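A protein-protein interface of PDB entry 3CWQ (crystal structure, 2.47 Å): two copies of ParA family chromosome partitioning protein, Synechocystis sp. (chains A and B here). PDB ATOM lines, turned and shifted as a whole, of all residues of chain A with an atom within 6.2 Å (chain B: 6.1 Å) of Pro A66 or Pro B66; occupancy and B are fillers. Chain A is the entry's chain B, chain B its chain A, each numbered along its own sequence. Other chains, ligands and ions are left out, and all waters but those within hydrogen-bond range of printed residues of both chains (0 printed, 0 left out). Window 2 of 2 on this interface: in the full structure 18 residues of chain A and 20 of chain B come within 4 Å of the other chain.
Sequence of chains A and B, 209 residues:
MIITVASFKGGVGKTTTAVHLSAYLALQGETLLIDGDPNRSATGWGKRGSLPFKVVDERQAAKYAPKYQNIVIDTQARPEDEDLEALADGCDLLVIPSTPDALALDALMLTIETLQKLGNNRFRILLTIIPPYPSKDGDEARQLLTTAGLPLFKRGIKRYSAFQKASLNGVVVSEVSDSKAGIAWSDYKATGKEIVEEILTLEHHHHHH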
ATOM      1  N   ALA A  61     -19.348  13.227  -9.656  1.00  0.00           N
ATOM      2  CA  ALA A  61     -20.772  13.659  -9.599  1.00  0.00           C
ATOM      3  C   ALA A  61     -21.528  12.520  -8.979  1.00  0.00           C
ATOM      4  O   ALA A  61     -22.283  12.730  -8.034  1.00  0.00           O
ATOM      5  CB  ALA A  61     -21.309  14.103 -11.008  1.00  0.00           C
ATOM      6  N   ALA A  62     -21.193  11.298  -9.370  1.00  0.00           N
ATOM      7  CA  ALA A  62     -22.004  10.157  -8.893  1.00  0.00           C
ATOM      8  C   ALA A  62     -21.718   9.909  -7.417  1.00  0.00           C
ATOM      9  O   ALA A  62     -22.600   9.568  -6.674  1.00  0.00           O
ATOM     10  CB  ALA A  62     -21.732   8.872  -9.729  1.00  0.00           C
ATOM     11  N   LYS A  63     -20.460  10.035  -7.021  1.00  0.00           N
ATOM     12  CA  LYS A  63     -20.098   9.866  -5.624  1.00  0.00           C
ATOM     13  C   LYS A  63     -20.800  10.922  -4.783  1.00  0.00           C
ATOM     14  O   LYS A  63     -21.532  10.552  -3.911  1.00  0.00           O
ATOM     15  CB  LYS A  63     -18.566   9.961  -5.446  1.00  0.00           C
ATOM     16  CG  LYS A  63     -18.108   9.815  -4.024  1.00  0.00           C
ATOM     17  CD  LYS A  63     -16.662  10.206  -3.971  1.00  0.00           C
ATOM     18  CE  LYS A  63     -16.008   9.893  -2.639  1.00  0.00           C
ATOM     19  NZ  LYS A  63     -15.398   8.497  -2.831  1.00  0.00           N
ATOM     20  N   TYR A  64     -20.650  12.233  -5.056  1.00  0.00           N
ATOM     21  CA  TYR A  64     -21.178  13.264  -4.108  1.00  0.00           C
ATOM     22  C   TYR A  64     -22.667  13.628  -4.258  1.00  0.00           C
ATOM     23  O   TYR A  64     -23.273  14.079  -3.276  1.00  0.00           O
ATOM     24  CB  TYR A  64     -20.360  14.540  -4.132  1.00  0.00           C
ATOM     25  CG  TYR A  64     -19.022  14.344  -3.637  1.00  0.00           C
ATOM     26  CD1 TYR A  64     -18.055  13.805  -4.444  1.00  0.00           C
ATOM     27  CD2 TYR A  64     -18.685  14.712  -2.331  1.00  0.00           C
ATOM     28  CE1 TYR A  64     -16.795  13.588  -3.970  1.00  0.00           C
ATOM     29  CE2 TYR A  64     -17.400  14.494  -1.820  1.00  0.00           C
ATOM     30  CZ  TYR A  64     -16.455  13.924  -2.656  1.00  0.00           C
ATOM     31  OH  TYR A  64     -15.160  13.679  -2.201  1.00  0.00           O
ATOM     32  N   ALA A  65     -23.246  13.475  -5.453  1.00  0.00           N
ATOM     33  CA  ALA A  65     -24.694  13.796  -5.696  1.00  0.00           C
ATOM     34  C   ALA A  65     -25.737  13.308  -4.691  1.00  0.00           C
ATOM     35  O   ALA A  65     -26.680  14.028  -4.446  1.00  0.00           O
ATOM     36  CB  ALA A  65     -25.146  13.328  -7.117  1.00  0.00           C
ATOM     37  N   PRO A  66     -25.667  12.078  -4.203  1.00  0.00           N
ATOM     38  CA  PRO A  66     -26.561  11.642  -3.120  1.00  0.00           C
ATOM     39  C   PRO A  66     -26.383  12.402  -1.813  1.00  0.00           C
ATOM     40  O   PRO A  66     -27.144  12.179  -0.910  1.00  0.00           O
ATOM     41  CB  PRO A  66     -26.129  10.171  -2.851  1.00  0.00           C
ATOM     42  CG  PRO A  66     -25.478   9.686  -4.086  1.00  0.00           C
ATOM     43  CD  PRO A  66     -24.811  10.958  -4.670  1.00  0.00           C
ATOM     44  N   LYS A  67     -25.367  13.225  -1.637  1.00  0.00           N
ATOM     45  CA  LYS A  67     -25.225  13.886  -0.315  1.00  0.00           C
ATOM     46  C   LYS A  67     -25.987  15.261  -0.157  1.00  0.00           C
ATOM     47  O   LYS A  67     -26.065  15.841   0.931  1.00  0.00           O
ATOM     48  CB  LYS A  67     -23.715  13.956   0.074  1.00  0.00           C
ATOM     49  CG  LYS A  67     -22.962  12.573   0.038  1.00  0.00           C
ATOM     50  CD  LYS A  67     -21.327  12.509   0.204  1.00  0.00           C
ATOM     51  CE  LYS A  67     -20.726  11.014   0.655  1.00  0.00           C
ATOM     52  NZ  LYS A  67     -19.250  10.653   0.319  1.00  0.00           N
ATOM     53  N   TYR A  68     -26.574  15.757  -1.231  1.00  0.00           N
ATOM     54  CA  TYR A  68     -26.928  17.225  -1.296  1.00  0.00           C
ATOM     55  C   TYR A  68     -28.369  17.433  -1.666  1.00  0.00           C
ATOM     56  O   TYR A  68     -28.866  16.805  -2.590  1.00  0.00           O
ATOM     57  CB  TYR A  68     -25.996  17.985  -2.290  1.00  0.00           C
ATOM     58  CG  TYR A  68     -24.594  18.154  -1.719  1.00  0.00           C
ATOM     59  CD1 TYR A  68     -23.630  17.111  -1.835  1.00  0.00           C
ATOM     60  CD2 TYR A  68     -24.263  19.262  -0.974  1.00  0.00           C
ATOM     61  CE1 TYR A  68     -22.354  17.227  -1.271  1.00  0.00           C
ATOM     62  CE2 TYR A  68     -22.992  19.390  -0.389  1.00  0.00           C
ATOM     63  CZ  TYR A  68     -22.064  18.361  -0.544  1.00  0.00           C
ATOM     64  OH  TYR A  68     -20.840  18.464   0.040  1.00  0.00           O
ATOM     65  N   ILE A  71     -28.219  20.837  -6.338  1.00  0.00           N
ATOM     66  CA  ILE A  71     -27.183  20.537  -7.296  1.00  0.00           C
ATOM     67  C   ILE A  71     -27.246  21.480  -8.457  1.00  0.00           C
ATOM     68  O   ILE A  71     -28.275  21.613  -9.135  1.00  0.00           O
ATOM     69  CB  ILE A  71     -27.332  19.047  -7.807  1.00  0.00           C
ATOM     70  CG1 ILE A  71     -27.405  18.070  -6.588  1.00  0.00           C
ATOM     71  CG2 ILE A  71     -26.196  18.703  -8.827  1.00  0.00           C
ATOM     72  CD1 ILE A  71     -27.411  16.587  -6.895  1.00  0.00           C
ATOM     73  N   ALA B  61     -26.085  11.558 -14.510  1.00  0.00           N
ATOM     74  CA  ALA B  61     -25.412  11.020 -13.345  1.00  0.00           C
ATOM     75  C   ALA B  61     -25.858  11.633 -12.063  1.00  0.00           C
ATOM     76  O   ALA B  61     -26.151  10.877 -11.178  1.00  0.00           O
ATOM     77  CB  ALA B  61     -23.878  11.071 -13.510  1.00  0.00           C
ATOM     78  N   ALA B  62     -25.962  12.955 -11.939  1.00  0.00           N
ATOM     79  CA  ALA B  62     -26.480  13.535 -10.655  1.00  0.00           C
ATOM     80  C   ALA B  62     -27.901  13.102 -10.302  1.00  0.00           C
ATOM     81  O   ALA B  62     -28.243  12.974  -9.132  1.00  0.00           O
ATOM     82  CB  ALA B  62     -26.444  15.056 -10.663  1.00  0.00           C
ATOM     83  N   LYS B  63     -28.748  12.932 -11.315  1.00  0.00           N
ATOM     84  CA  LYS B  63     -30.169  12.736 -11.120  1.00  0.00           C
ATOM     85  C   LYS B  63     -30.369  11.321 -10.647  1.00  0.00           C
ATOM     86  O   LYS B  63     -30.967  11.105  -9.600  1.00  0.00           O
ATOM     87  CB  LYS B  63     -30.909  12.930 -12.414  1.00  0.00           C
ATOM     88  CG  LYS B  63     -32.393  12.481 -12.397  1.00  0.00           C
ATOM     89  CD  LYS B  63     -33.147  13.034 -13.637  1.00  0.00           C
ATOM     90  CE  LYS B  63     -34.692  12.854 -13.595  1.00  0.00           C
ATOM     91  NZ  LYS B  63     -35.128  12.462 -14.948  1.00  0.00           N
ATOM     92  N   TYR B  64     -29.792  10.378 -11.397  1.00  0.00           N
ATOM     93  CA  TYR B  64     -29.890   8.920 -11.158  1.00  0.00           C
ATOM     94  C   TYR B  64     -29.002   8.243 -10.124  1.00  0.00           C
ATOM     95  O   TYR B  64     -29.350   7.152  -9.691  1.00  0.00           O
ATOM     96  CB  TYR B  64     -29.727   8.169 -12.488  1.00  0.00           C
ATOM     97  CG  TYR B  64     -30.898   8.393 -13.393  1.00  0.00           C
ATOM     98  CD1 TYR B  64     -30.976   9.551 -14.163  1.00  0.00           C
ATOM     99  CD2 TYR B  64     -31.949   7.480 -13.459  1.00  0.00           C
ATOM    100  CE1 TYR B  64     -32.075   9.797 -15.004  1.00  0.00           C
ATOM    101  CE2 TYR B  64     -33.052   7.708 -14.313  1.00  0.00           C
ATOM    102  CZ  TYR B  64     -33.097   8.887 -15.074  1.00  0.00           C
ATOM    103  OH  TYR B  64     -34.151   9.207 -15.913  1.00  0.00           O
ATOM    104  N   ALA B  65     -27.882   8.853  -9.718  1.00  0.00           N
ATOM    105  CA  ALA B  65     -26.893   8.160  -8.905  1.00  0.00           C
ATOM    106  C   ALA B  65     -27.403   7.828  -7.501  1.00  0.00           C
ATOM    107  O   ALA B  65     -27.016   6.806  -6.938  1.00  0.00           O
ATOM    108  CB  ALA B  65     -25.640   8.926  -8.853  1.00  0.00           C
ATOM    109  N   PRO B  66     -28.274   8.650  -6.915  1.00  0.00           N
ATOM    110  CA  PRO B  66     -28.649   8.405  -5.534  1.00  0.00           C
ATOM    111  C   PRO B  66     -29.636   7.278  -5.422  1.00  0.00           C
ATOM    112  O   PRO B  66     -29.866   6.743  -4.345  1.00  0.00           O
ATOM    113  CB  PRO B  66     -29.251   9.739  -5.061  1.00  0.00           C
ATOM    114  CG  PRO B  66     -29.725  10.376  -6.252  1.00  0.00           C
ATOM    115  CD  PRO B  66     -28.925   9.853  -7.454  1.00  0.00           C
ATOM    116  N   LYS B  67     -30.188   6.863  -6.535  1.00  0.00           N
ATOM    117  CA  LYS B  67     -31.124   5.749  -6.468  1.00  0.00           C
ATOM    118  C   LYS B  67     -30.449   4.381  -6.645  1.00  0.00           C
ATOM    119  O   LYS B  67     -31.180   3.383  -6.648  1.00  0.00           O
ATOM    120  CB  LYS B  67     -32.257   5.937  -7.478  1.00  0.00           C
ATOM    121  CG  LYS B  67     -33.300   6.912  -6.983  1.00  0.00           C
ATOM    122  CD  LYS B  67     -33.652   7.981  -8.012  1.00  0.00           C
ATOM    123  CE  LYS B  67     -34.925   8.782  -7.596  1.00  0.00           C
ATOM    124  NZ  LYS B  67     -34.848   9.594  -6.295  1.00  0.00           N
ATOM    125  N   TYR B  68     -29.104   4.308  -6.775  1.00  0.00           N
ATOM    126  CA  TYR B  68     -28.398   3.014  -7.028  1.00  0.00           C
ATOM    127  C   TYR B  68     -27.334   2.591  -6.050  1.00  0.00           C
ATOM    128  O   TYR B  68     -26.579   3.412  -5.559  1.00  0.00           O
ATOM    129  CB  TYR B  68     -27.857   2.899  -8.460  1.00  0.00           C
ATOM    130  CG  TYR B  68     -28.985   2.840  -9.443  1.00  0.00           C
ATOM    131  CD1 TYR B  68     -29.557   4.011  -9.956  1.00  0.00           C
ATOM    132  CD2 TYR B  68     -29.545   1.639  -9.794  1.00  0.00           C
ATOM    133  CE1 TYR B  68     -30.649   3.966 -10.855  1.00  0.00           C
ATOM    134  CE2 TYR B  68     -30.618   1.562 -10.701  1.00  0.00           C
ATOM    135  CZ  TYR B  68     -31.157   2.731 -11.216  1.00  0.00           C
ATOM    136  OH  TYR B  68     -32.213   2.638 -12.080  1.00  0.00           O
ATOM    137  N   ILE B  71     -22.496   1.688  -8.751  1.00  0.00           N
ATOM    138  CA  ILE B  71     -22.363   2.499  -9.991  1.00  0.00           C
ATOM    139  C   ILE B  71     -21.099   2.077 -10.721  1.00  0.00           C
ATOM    140  O   ILE B  71     -20.030   2.025 -10.091  1.00  0.00           O
ATOM    141  CB  ILE B  71     -22.399   4.004  -9.613  1.00  0.00           C
ATOM    142  CG1 ILE B  71     -23.743   4.269  -8.973  1.00  0.00           C
ATOM    143  CG2 ILE B  71     -22.427   4.893 -10.790  1.00  0.00           C
ATOM    144  CD1 ILE B  71     -23.749   5.482  -8.209  1.00  0.00           C
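Of the 9 printed residues of chain A, 3 touch a printed residue of chain B.
Printed residues of chain A that touch a printed residue of chain B: Ala A62, Ala A65 and Pro A66.
Hydrophobic or aromatic side chains of chain A that line the printed part of chain B: Ala A65 and Pro A66.
Among the printed residues, 3 pairs touch across the chains.
Among the printed residues, no Asp or Glu carboxylate lies within 4 Å of a Lys or Arg side-chain nitrogen of the other chain.
Ala A62 touches Ala B65, and with the chains exchanged Ala A65 touches Ala B62.
Pro B66 touches its own counterpart, Pro A66.
Pro A66 touches just one residue of chain B: Pro B66.
Of the printed residues of chain A, Ala B62 touches Ala A65 (3.7 Å).
Lys B63 touches none of the printed residues of chain A.
Of the printed residues of chain A, Ala B65 touches Ala A62 (3.8 Å).
Of the printed residues of chain A, Pro B66 touches Pro A66 (3.7 Å).
The nearest residue of chain B that does not touch Pro A66 is Ala B65 (4.3 Å).
Ala A62 touches Ala B65 (O to CB, 3.8 Å).
Ala A65 touches Ala B62.
CG of Pro A66 touches CA of Pro B66, at 3.7 Å.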
